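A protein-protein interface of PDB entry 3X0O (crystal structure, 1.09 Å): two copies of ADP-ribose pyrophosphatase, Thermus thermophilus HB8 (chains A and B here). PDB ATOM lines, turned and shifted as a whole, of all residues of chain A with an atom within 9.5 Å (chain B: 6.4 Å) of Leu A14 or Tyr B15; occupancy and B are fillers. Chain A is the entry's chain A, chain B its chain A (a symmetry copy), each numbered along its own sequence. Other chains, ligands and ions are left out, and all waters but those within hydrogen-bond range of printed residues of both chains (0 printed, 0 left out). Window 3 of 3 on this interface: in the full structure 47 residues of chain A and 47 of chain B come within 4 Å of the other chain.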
ATOM      1  N   ARG A  11      17.162   8.184  10.538  1.00  0.00           N
ATOM      2  CA  ARG A  11      17.744   9.019   9.491  1.00  0.00           C
ATOM      3  C   ARG A  11      17.576  10.505   9.765  1.00  0.00           C
ATOM      4  O   ARG A  11      16.520  10.951  10.175  1.00  0.00           O
ATOM      5  CB  ARG A  11      17.107   8.644   8.136  1.00  0.00           C
ATOM      6  CG  ARG A  11      17.658   7.300   7.733  1.00  0.00           C
ATOM      7  CD  ARG A  11      16.941   6.891   6.428  1.00  0.00           C
ATOM      8  NE  ARG A  11      17.473   5.535   6.196  1.00  0.00           N
ATOM      9  CZ  ARG A  11      17.175   4.758   5.195  1.00  0.00           C
ATOM     10  NH1 ARG A  11      16.308   5.259   4.305  1.00  0.00           N
ATOM     11  NH2 ARG A  11      17.718   3.550   5.075  1.00  0.00           N
ATOM     12  N   THR A  12      18.657  11.202   9.513  1.00  0.00           N
ATOM     13  CA  THR A  12      18.700  12.655   9.479  1.00  0.00           C
ATOM     14  C   THR A  12      18.902  13.035   8.020  1.00  0.00           C
ATOM     15  O   THR A  12      19.747  12.531   7.289  1.00  0.00           O
ATOM     16  CB  THR A  12      19.786  13.162  10.421  1.00  0.00           C
ATOM     17  OG1 THR A  12      21.096  12.989   9.881  1.00  0.00           O
ATOM     18  CG2 THR A  12      19.777  12.315  11.701  1.00  0.00           C
ATOM     19  N   TYR A  13      18.061  13.930   7.528  1.00  0.00           N
ATOM     20  CA  TYR A  13      18.043  14.305   6.136  1.00  0.00           C
ATOM     21  C   TYR A  13      18.908  15.522   5.917  1.00  0.00           C
ATOM     22  O   TYR A  13      18.776  16.538   6.626  1.00  0.00           O
ATOM     23  CB  TYR A  13      16.577  14.527   5.652  1.00  0.00           C
ATOM     24  CG  TYR A  13      15.949  13.127   5.617  1.00  0.00           C
ATOM     25  CD1 TYR A  13      15.303  12.584   6.714  1.00  0.00           C
ATOM     26  CD2 TYR A  13      16.048  12.344   4.477  1.00  0.00           C
ATOM     27  CE1 TYR A  13      14.752  11.316   6.673  1.00  0.00           C
ATOM     28  CE2 TYR A  13      15.495  11.060   4.423  1.00  0.00           C
ATOM     29  CZ  TYR A  13      14.849  10.561   5.524  1.00  0.00           C
ATOM     30  OH  TYR A  13      14.292   9.307   5.540  1.00  0.00           O
ATOM     31  N   LEU A  14      19.785  15.413   4.955  1.00  0.00           N
ATOM     32  CA  LEU A  14      20.622  16.518   4.559  1.00  0.00           C
ATOM     33  C   LEU A  14      20.058  17.207   3.314  1.00  0.00           C
ATOM     34  O   LEU A  14      20.336  18.394   3.136  1.00  0.00           O
ATOM     35  CB  LEU A  14      22.063  16.040   4.296  1.00  0.00           C
ATOM     36  CG  LEU A  14      22.684  15.252   5.425  1.00  0.00           C
ATOM     37  CD1 LEU A  14      24.127  14.893   5.158  1.00  0.00           C
ATOM     38  CD2 LEU A  14      22.611  16.089   6.703  1.00  0.00           C
ATOM     39  N   TYR A  15      19.328  16.493   2.453  1.00  0.00           N
ATOM     40  CA  TYR A  15      18.849  17.048   1.186  1.00  0.00           C
ATOM     41  C   TYR A  15      17.611  16.243   0.842  1.00  0.00           C
ATOM     42  O   TYR A  15      17.667  15.009   0.861  1.00  0.00           O
ATOM     43  CB  TYR A  15      19.904  16.966   0.082  1.00  0.00           C
ATOM     44  CG  TYR A  15      19.349  17.399  -1.260  1.00  0.00           C
ATOM     45  CD1 TYR A  15      19.156  18.740  -1.582  1.00  0.00           C
ATOM     46  CD2 TYR A  15      18.978  16.480  -2.251  1.00  0.00           C
ATOM     47  CE1 TYR A  15      18.649  19.171  -2.790  1.00  0.00           C
ATOM     48  CE2 TYR A  15      18.459  16.852  -3.502  1.00  0.00           C
ATOM     49  CZ  TYR A  15      18.308  18.212  -3.743  1.00  0.00           C
ATOM     50  OH  TYR A  15      17.807  18.663  -4.919  1.00  0.00           O
ATOM     51  N   ARG A  16      16.484  16.846   0.557  1.00  0.00           N
ATOM     52  CA  ARG A  16      15.272  16.255   0.007  1.00  0.00           C
ATOM     53  C   ARG A  16      15.073  16.797  -1.407  1.00  0.00           C
ATOM     54  O   ARG A  16      14.817  17.996  -1.509  1.00  0.00           O
ATOM     55  CB  ARG A  16      14.069  16.592   0.875  1.00  0.00           C
ATOM     56  CG  ARG A  16      14.050  15.782   2.184  1.00  0.00           C
ATOM     57  CD  ARG A  16      12.669  15.995   2.787  1.00  0.00           C
ATOM     58  NE  ARG A  16      12.496  15.231   4.015  1.00  0.00           N
ATOM     59  CZ  ARG A  16      12.248  13.922   4.054  1.00  0.00           C
ATOM     60  NH1 ARG A  16      12.144  13.210   2.936  1.00  0.00           N
ATOM     61  NH2 ARG A  16      12.110  13.333   5.252  1.00  0.00           N
ATOM     62  N   GLY A  17      15.179  15.983  -2.440  1.00  0.00           N
ATOM     63  CA  GLY A  17      15.135  16.405  -3.815  1.00  0.00           C
ATOM     64  C   GLY A  17      13.991  15.813  -4.619  1.00  0.00           C
ATOM     65  O   GLY A  17      12.976  15.314  -4.132  1.00  0.00           O
ATOM     66  N   LEU A  20      15.834  12.092  -5.493  1.00  0.00           N
ATOM     67  CA  LEU A  20      16.539  11.439  -4.381  1.00  0.00           C
ATOM     68  C   LEU A  20      16.489  12.271  -3.106  1.00  0.00           C
ATOM     69  O   LEU A  20      16.282  13.483  -3.188  1.00  0.00           O
ATOM     70  CB  LEU A  20      17.976  11.108  -4.796  1.00  0.00           C
ATOM     71  CG  LEU A  20      18.932  12.252  -5.106  1.00  0.00           C
ATOM     72  CD1 LEU A  20      19.587  12.871  -3.887  1.00  0.00           C
ATOM     73  CD2 LEU A  20      20.017  11.779  -6.105  1.00  0.00           C
ATOM     74  N   ASN A  21      16.722  11.613  -1.976  1.00  0.00           N
ATOM     75  CA  ASN A  21      16.971  12.244  -0.707  1.00  0.00           C
ATOM     76  C   ASN A  21      18.364  11.762  -0.252  1.00  0.00           C
ATOM     77  O   ASN A  21      18.706  10.603  -0.501  1.00  0.00           O
ATOM     78  CB  ASN A  21      15.978  11.913   0.380  1.00  0.00           C
ATOM     79  CG  ASN A  21      14.532  12.204  -0.046  1.00  0.00           C
ATOM     80  OD1 ASN A  21      14.325  13.252  -0.684  1.00  0.00           O
ATOM     81  ND2 ASN A  21      13.706  11.243   0.359  1.00  0.00           N
ATOM     82  N   LEU A  22      19.129  12.631   0.436  1.00  0.00           N
ATOM     83  CA  LEU A  22      20.350  12.215   1.073  1.00  0.00           C
ATOM     84  C   LEU A  22      20.178  12.250   2.586  1.00  0.00           C
ATOM     85  O   LEU A  22      19.765  13.302   3.115  1.00  0.00           O
ATOM     86  CB  LEU A  22      21.544  13.114   0.681  1.00  0.00           C
ATOM     87  CG  LEU A  22      22.818  12.856   1.483  1.00  0.00           C
ATOM     88  CD1 LEU A  22      23.381  11.437   1.220  1.00  0.00           C
ATOM     89  CD2 LEU A  22      23.851  13.894   1.130  1.00  0.00           C
ATOM     90  N   ALA A  23      20.497  11.131   3.222  1.00  0.00           N
ATOM     91  CA  ALA A  23      20.323  11.022   4.663  1.00  0.00           C
ATOM     92  C   ALA A  23      21.595  10.472   5.293  1.00  0.00           C
ATOM     93  O   ALA A  23      22.343   9.771   4.627  1.00  0.00           O
ATOM     94  CB  ALA A  23      19.089  10.172   5.018  1.00  0.00           C
ATOM     95  N   LEU A  24      21.769  10.729   6.569  1.00  0.00           N
ATOM     96  CA  LEU A  24      22.767  10.022   7.357  1.00  0.00           C
ATOM     97  C   LEU A  24      22.048   9.129   8.366  1.00  0.00           C
ATOM     98  O   LEU A  24      21.053   9.488   9.021  1.00  0.00           O
ATOM     99  CB  LEU A  24      23.626  11.012   8.164  1.00  0.00           C
ATOM    100  CG  LEU A  24      24.317  12.098   7.332  1.00  0.00           C
ATOM    101  CD1 LEU A  24      25.104  13.027   8.260  1.00  0.00           C
ATOM    102  CD2 LEU A  24      25.193  11.538   6.230  1.00  0.00           C
ATOM    103  N   GLU A  25      22.569   7.922   8.496  1.00  0.00           N
ATOM    104  CA  GLU A  25      22.033   7.003   9.492  1.00  0.00           C
ATOM    105  C   GLU A  25      23.239   6.492  10.242  1.00  0.00           C
ATOM    106  O   GLU A  25      23.972   5.661   9.698  1.00  0.00           O
ATOM    107  CB  GLU A  25      21.297   5.954   8.707  1.00  0.00           C
ATOM    108  CG  GLU A  25      20.694   4.863   9.507  1.00  0.00           C
ATOM    109  CD  GLU A  25      19.911   3.844   8.759  1.00  0.00           C
ATOM    110  OE1 GLU A  25      19.298   3.982   7.673  1.00  0.00           O
ATOM    111  OE2 GLU A  25      19.915   2.731   9.324  1.00  0.00           O
ATOM    112  N   GLY A  26      23.449   7.097  11.413  1.00  0.00           N
ATOM    113  CA  GLY A  26      24.718   6.874  12.101  1.00  0.00           C
ATOM    114  C   GLY A  26      25.882   7.217  11.188  1.00  0.00           C
ATOM    115  O   GLY A  26      25.938   8.353  10.702  1.00  0.00           O
ATOM    116  N   ARG A  27      26.797   6.243  10.928  1.00  0.00           N
ATOM    117  CA  ARG A  27      27.897   6.681  10.073  1.00  0.00           C
ATOM    118  C   ARG A  27      27.618   6.477   8.590  1.00  0.00           C
ATOM    119  O   ARG A  27      28.446   6.805   7.714  1.00  0.00           O
ATOM    120  CB  ARG A  27      29.164   5.919  10.435  1.00  0.00           C
ATOM    121  N   TYR A  28      26.457   5.940   8.275  1.00  0.00           N
ATOM    122  CA  TYR A  28      26.159   5.571   6.897  1.00  0.00           C
ATOM    123  C   TYR A  28      25.568   6.711   6.123  1.00  0.00           C
ATOM    124  O   TYR A  28      24.677   7.415   6.604  1.00  0.00           O
ATOM    125  CB  TYR A  28      25.182   4.385   6.884  1.00  0.00           C
ATOM    126  CG  TYR A  28      25.883   3.102   7.267  1.00  0.00           C
ATOM    127  CD1 TYR A  28      26.386   2.181   6.364  1.00  0.00           C
ATOM    128  CD2 TYR A  28      25.991   2.828   8.615  1.00  0.00           C
ATOM    129  CE1 TYR A  28      26.999   1.023   6.857  1.00  0.00           C
ATOM    130  CE2 TYR A  28      26.606   1.693   9.143  1.00  0.00           C
ATOM    131  CZ  TYR A  28      27.107   0.781   8.228  1.00  0.00           C
ATOM    132  OH  TYR A  28      27.733  -0.351   8.743  1.00  0.00           O
ATOM    133  N   GLU A  29      26.033   6.922   4.903  1.00  0.00           N
ATOM    134  CA  GLU A  29      25.449   7.917   3.979  1.00  0.00           C
ATOM    135  C   GLU A  29      24.494   7.127   3.082  1.00  0.00           C
ATOM    136  O   GLU A  29      24.890   6.146   2.414  1.00  0.00           O
ATOM    137  CB  GLU A  29      26.580   8.548   3.205  1.00  0.00           C
ATOM    138  CG  GLU A  29      27.572   9.251   4.103  1.00  0.00           C
ATOM    139  CD  GLU A  29      28.941   9.464   3.462  1.00  0.00           C
ATOM    140  OE1 GLU A  29      29.355   8.854   2.457  1.00  0.00           O
ATOM    141  OE2 GLU A  29      29.611  10.319   4.051  1.00  0.00           O
ATOM    142  N   ILE A  30      23.238   7.540   3.048  1.00  0.00           N
ATOM    143  CA  ILE A  30      22.197   6.804   2.367  1.00  0.00           C
ATOM    144  C   ILE A  30      21.423   7.681   1.433  1.00  0.00           C
ATOM    145  O   ILE A  30      20.974   8.751   1.802  1.00  0.00           O
ATOM    146  CB  ILE A  30      21.190   6.234   3.399  1.00  0.00           C
ATOM    147  CG1 ILE A  30      21.879   5.235   4.327  1.00  0.00           C
ATOM    148  CG2 ILE A  30      19.980   5.678   2.668  1.00  0.00           C
ATOM    149  CD1 ILE A  30      22.774   4.252   3.587  1.00  0.00           C
ATOM    150  N   VAL A  31      21.309   7.218   0.200  1.00  0.00           N
ATOM    151  CA  VAL A  31      20.525   7.912  -0.829  1.00  0.00           C
ATOM    152  C   VAL A  31      19.259   7.162  -1.032  1.00  0.00           C
ATOM    153  O   VAL A  31      19.269   6.050  -1.568  1.00  0.00           O
ATOM    154  CB  VAL A  31      21.321   8.035  -2.127  1.00  0.00           C
ATOM    155  CG1 VAL A  31      20.400   8.704  -3.169  1.00  0.00           C
ATOM    156  CG2 VAL A  31      22.544   8.926  -1.901  1.00  0.00           C
ATOM    157  N   GLU A  32      18.125   7.784  -0.672  1.00  0.00           N
ATOM    158  CA  GLU A  32      16.794   7.258  -0.985  1.00  0.00           C
ATOM    159  C   GLU A  32      16.449   7.670  -2.406  1.00  0.00           C
ATOM    160  O   GLU A  32      16.680   8.790  -2.802  1.00  0.00           O
ATOM    161  CB  GLU A  32      15.769   7.844  -0.009  1.00  0.00           C
ATOM    162  CG  GLU A  32      15.925   7.343   1.419  1.00  0.00           C
ATOM    163  CD  GLU A  32      15.078   8.011   2.453  1.00  0.00           C
ATOM    164  OE1 GLU A  32      14.297   8.988   2.009  1.00  0.00           O
ATOM    165  OE2 GLU A  32      15.138   7.718   3.621  1.00  0.00           O
ATOM    166  N   THR B  12      27.763  22.191  -8.272  1.00  0.00           N
ATOM    167  CA  THR B  12      27.723  22.809  -6.956  1.00  0.00           C
ATOM    168  C   THR B  12      27.519  21.674  -5.965  1.00  0.00           C
ATOM    169  O   THR B  12      26.673  20.798  -6.088  1.00  0.00           O
ATOM    170  CB  THR B  12      26.639  23.881  -6.922  1.00  0.00           C
ATOM    171  OG1 THR B  12      25.328  23.323  -6.833  1.00  0.00           O
ATOM    172  CG2 THR B  12      26.648  24.648  -8.252  1.00  0.00           C
ATOM    173  N   TYR B  13      28.362  21.632  -4.945  1.00  0.00           N
ATOM    174  CA  TYR B  13      28.379  20.553  -3.988  1.00  0.00           C
ATOM    175  C   TYR B  13      27.517  20.903  -2.801  1.00  0.00           C
ATOM    176  O   TYR B  13      27.652  21.990  -2.208  1.00  0.00           O
ATOM    177  CB  TYR B  13      29.845  20.217  -3.575  1.00  0.00           C
ATOM    178  CG  TYR B  13      30.470  19.559  -4.814  1.00  0.00           C
ATOM    179  CD1 TYR B  13      31.116  20.297  -5.790  1.00  0.00           C
ATOM    180  CD2 TYR B  13      30.368  18.189  -5.005  1.00  0.00           C
ATOM    181  CE1 TYR B  13      31.665  19.693  -6.907  1.00  0.00           C
ATOM    182  CE2 TYR B  13      30.918  17.567  -6.130  1.00  0.00           C
ATOM    183  CZ  TYR B  13      31.564  18.327  -7.069  1.00  0.00           C
ATOM    184  OH  TYR B  13      32.119  17.781  -8.199  1.00  0.00           O
ATOM    185  N   LEU B  14      26.637  19.995  -2.468  1.00  0.00           N
ATOM    186  CA  LEU B  14      25.803  20.136  -1.302  1.00  0.00           C
ATOM    187  C   LEU B  14      26.366  19.328  -0.129  1.00  0.00           C
ATOM    188  O   LEU B  14      26.090  19.700   1.013  1.00  0.00           O
ATOM    189  CB  LEU B  14      24.360  19.690  -1.609  1.00  0.00           C
ATOM    190  CG  LEU B  14      23.739  20.349  -2.818  1.00  0.00           C
ATOM    191  CD1 LEU B  14      22.295  19.953  -3.018  1.00  0.00           C
ATOM    192  CD2 LEU B  14      23.816  21.866  -2.640  1.00  0.00           C
ATOM    193  N   TYR B  15      27.094  18.238  -0.385  1.00  0.00           N
ATOM    194  CA  TYR B  15      27.572  17.350   0.677  1.00  0.00           C
ATOM    195  C   TYR B  15      28.808  16.680   0.109  1.00  0.00           C
ATOM    196  O   TYR B  15      28.749  16.147  -1.004  1.00  0.00           O
ATOM    197  CB  TYR B  15      26.516  16.328   1.097  1.00  0.00           C
ATOM    198  CG  TYR B  15      27.071  15.319   2.084  1.00  0.00           C
ATOM    199  CD1 TYR B  15      27.265  15.630   3.427  1.00  0.00           C
ATOM    200  CD2 TYR B  15      27.439  14.022   1.703  1.00  0.00           C
ATOM    201  CE1 TYR B  15      27.771  14.740   4.352  1.00  0.00           C
ATOM    202  CE2 TYR B  15      27.956  13.067   2.594  1.00  0.00           C
ATOM    203  CZ  TYR B  15      28.109  13.459   3.918  1.00  0.00           C
ATOM    204  OH  TYR B  15      28.609  12.607   4.847  1.00  0.00           O
ATOM    205  N   ARG B  16      29.936  16.693   0.774  1.00  0.00           N
ATOM    206  CA  ARG B  16      31.147  15.934   0.490  1.00  0.00           C
ATOM    207  C   ARG B  16      31.344  14.910   1.605  1.00  0.00           C
ATOM    208  O   ARG B  16      31.603  15.354   2.723  1.00  0.00           O
ATOM    209  CB  ARG B  16      32.351  16.859   0.402  1.00  0.00           C
ATOM    210  CG  ARG B  16      32.370  17.668  -0.908  1.00  0.00           C
ATOM    211  CD  ARG B  16      33.752  18.301  -0.988  1.00  0.00           C
ATOM    212  NE  ARG B  16      33.925  19.058  -2.220  1.00  0.00           N
ATOM    213  CZ  ARG B  16      34.171  18.508  -3.409  1.00  0.00           C
ATOM    214  NH1 ARG B  16      34.272  17.190  -3.547  1.00  0.00           N
ATOM    215  NH2 ARG B  16      34.309  19.317  -4.471  1.00  0.00           N
ATOM    216  N   GLY B  17      31.235  13.623   1.339  1.00  0.00           N
ATOM    217  CA  GLY B  17      31.278  12.581   2.330  1.00  0.00           C
ATOM    218  C   GLY B  17      32.421  11.595   2.158  1.00  0.00           C
ATOM    219  O   GLY B  17      33.435  11.806   1.493  1.00  0.00           O
ATOM    220  N   ARG B  18      32.137  10.488   2.849  1.00  0.00           N
ATOM    221  CA  ARG B  18      33.111   9.442   2.972  1.00  0.00           C
ATOM    222  C   ARG B  18      33.153   8.546   1.760  1.00  0.00           C
ATOM    223  O   ARG B  18      34.218   8.198   1.279  1.00  0.00           O
ATOM    224  CB  ARG B  18      32.758   8.632   4.249  1.00  0.00           C
ATOM    225  CG  ARG B  18      33.163   9.351   5.414  1.00  0.00           C
ATOM    226  N   LEU B  20      30.570   9.156  -0.780  1.00  0.00           N
ATOM    227  CA  LEU B  20      29.864   9.861  -1.859  1.00  0.00           C
ATOM    228  C   LEU B  20      29.918  11.373  -1.684  1.00  0.00           C
ATOM    229  O   LEU B  20      30.127  11.840  -0.563  1.00  0.00           O
ATOM    230  CB  LEU B  20      28.426   9.344  -1.968  1.00  0.00           C
ATOM    231  CG  LEU B  20      27.471   9.580  -0.806  1.00  0.00           C
ATOM    232  CD1 LEU B  20      26.820  10.948  -0.795  1.00  0.00           C
ATOM    233  CD2 LEU B  20      26.384   8.476  -0.781  1.00  0.00           C
ATOM    234  N   ASN B  21      29.684  12.091  -2.776  1.00  0.00           N
ATOM    235  CA  ASN B  21      29.439  13.508  -2.779  1.00  0.00           C
ATOM    236  C   ASN B  21      28.045  13.704  -3.411  1.00  0.00           C
ATOM    237  O   ASN B  21      27.700  12.963  -4.338  1.00  0.00           O
ATOM    238  CB  ASN B  21      30.432  14.331  -3.562  1.00  0.00           C
ATOM    239  CG  ASN B  21      31.878  14.077  -3.113  1.00  0.00           C
ATOM    240  OD1 ASN B  21      32.087  13.974  -1.890  1.00  0.00           O
ATOM    241  ND2 ASN B  21      32.702  14.008  -4.155  1.00  0.00           N
ATOM    242  N   LEU B  22      27.283  14.708  -2.941  1.00  0.00           N
ATOM    243  CA  LEU B  22      26.061  15.095  -3.596  1.00  0.00           C
ATOM    244  C   LEU B  22      26.235  16.463  -4.240  1.00  0.00           C
ATOM    245  O   LEU B  22      26.651  17.406  -3.535  1.00  0.00           O
ATOM    246  CB  LEU B  22      24.869  15.148  -2.614  1.00  0.00           C
ATOM    247  CG  LEU B  22      23.595  15.752  -3.202  1.00  0.00           C
ATOM    248  CD1 LEU B  22      23.029  14.885  -4.353  1.00  0.00           C
ATOM    249  CD2 LEU B  22      22.564  15.903  -2.114  1.00  0.00           C
ATOM    250  N   ALA B  23      25.915  16.533  -5.524  1.00  0.00           N
ATOM    251  CA  ALA B  23      26.091  17.774  -6.266  1.00  0.00           C
ATOM    252  C   ALA B  23      24.819  18.096  -7.037  1.00  0.00           C
ATOM    253  O   ALA B  23      24.068  17.187  -7.366  1.00  0.00           O
ATOM    254  CB  ALA B  23      27.323  17.710  -7.186  1.00  0.00           C
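O of Thr A12 lies within hydrogen-bond range of N of Leu A24 (2.8 Å).
The backbone NH (N) of Leu A14 is in hydrogen-bond range of the backbone carbonyl oxygen (O) of Leu A22, at 2.8 Å.
The backbone carbonyl oxygen (O) of Tyr A15 sits at hydrogen-bond distance from the backbone NH (N) of Leu A22.
The backbone carbonyl oxygen (O) of Leu B22 sits at hydrogen-bond distance from the backbone NH (N) of Leu B14 (2.8 Å).
The backbone carbonyl oxygen (O) of Tyr B15 sits at hydrogen-bond distance from the backbone NH (N) of Leu B22, at 2.8 Å.
OD1 of Asn B21 is in hydrogen-bond range of N of Gly B17.
Printed residues of chain B that touch a printed residue of chain A: Leu B14, Tyr B15, Gly B17, Arg B18, Leu B20 and Leu B22.
Hydrophobic or aromatic side chains of chain B that line the printed part of chain A: Leu B14, Tyr B15, Leu B20 and Leu B22.
Printed residues of chain A that touch a printed residue of chain B: Leu A14, Tyr A15, Leu A22, Leu A24 and Glu A29.
Along chain A the printed residues that touch a printed residue of chain B span positions 14 to 29.
Among the printed residues, no Asp or Glu carboxylate lies within 4 Å of a Lys or Arg side-chain nitrogen of the other chain.
Of the printed residues of chain B, Leu A14 touches Tyr B15.
Of the printed residues of chain B, Leu A24 touches Tyr B15 (3.8 Å).
Of the printed residues of chain A, Leu B22 touches Tyr A15 (3.6 Å).
Of the printed residues of chain B, Tyr A15 touches Leu B14 (3.7 Å) and Leu B22 (3.6 Å).
Printed residues of chain A within 4 Å of Leu B20: Glu A29.
Ile A30 touches none of the printed residues of chain B.
Glu A25 touches none of the printed residues of chain B.
The nearest printed residue of chain B that does not touch Leu A24 is Leu B20 (7.2 Å).
OH of Tyr B15 is in hydrogen-bond range of OE2 of Glu A29 (2.6 Å).
The side-chain carboxylate (OE2) of Glu A29 lies within hydrogen-bond range of the backbone NH (N) of Arg B18 (2.8 Å).
The side-chain carboxylate (OE1) of Glu A29 lies within hydrogen-bond range of the backbone NH (N) of Leu B20 (3.5 Å).
Leu A14 touches Tyr B15, and with the chains exchanged Tyr A15 touches Leu B14.
Tyr A15 touches Leu B22, and with the chains exchanged Leu A22 touches Tyr B15.
Of the 9 pairs that touch across the chains among the printed residues, 4 have their exchanged pair printed and touching as well.
Leu A14 touches Tyr B15.
CD1 of Leu B14 touches CD1 of Tyr A15 (3.7 Å).
Leu B22 touches Tyr A15.
CD2 of Leu A22 touches CB of Tyr B15, 3.6 Å away.
OH of Tyr B15 touches CD2 of Leu A24, 3.8 Å away.
OE2 of Glu A29 touches CA of Gly B17, at 3.3 Å.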
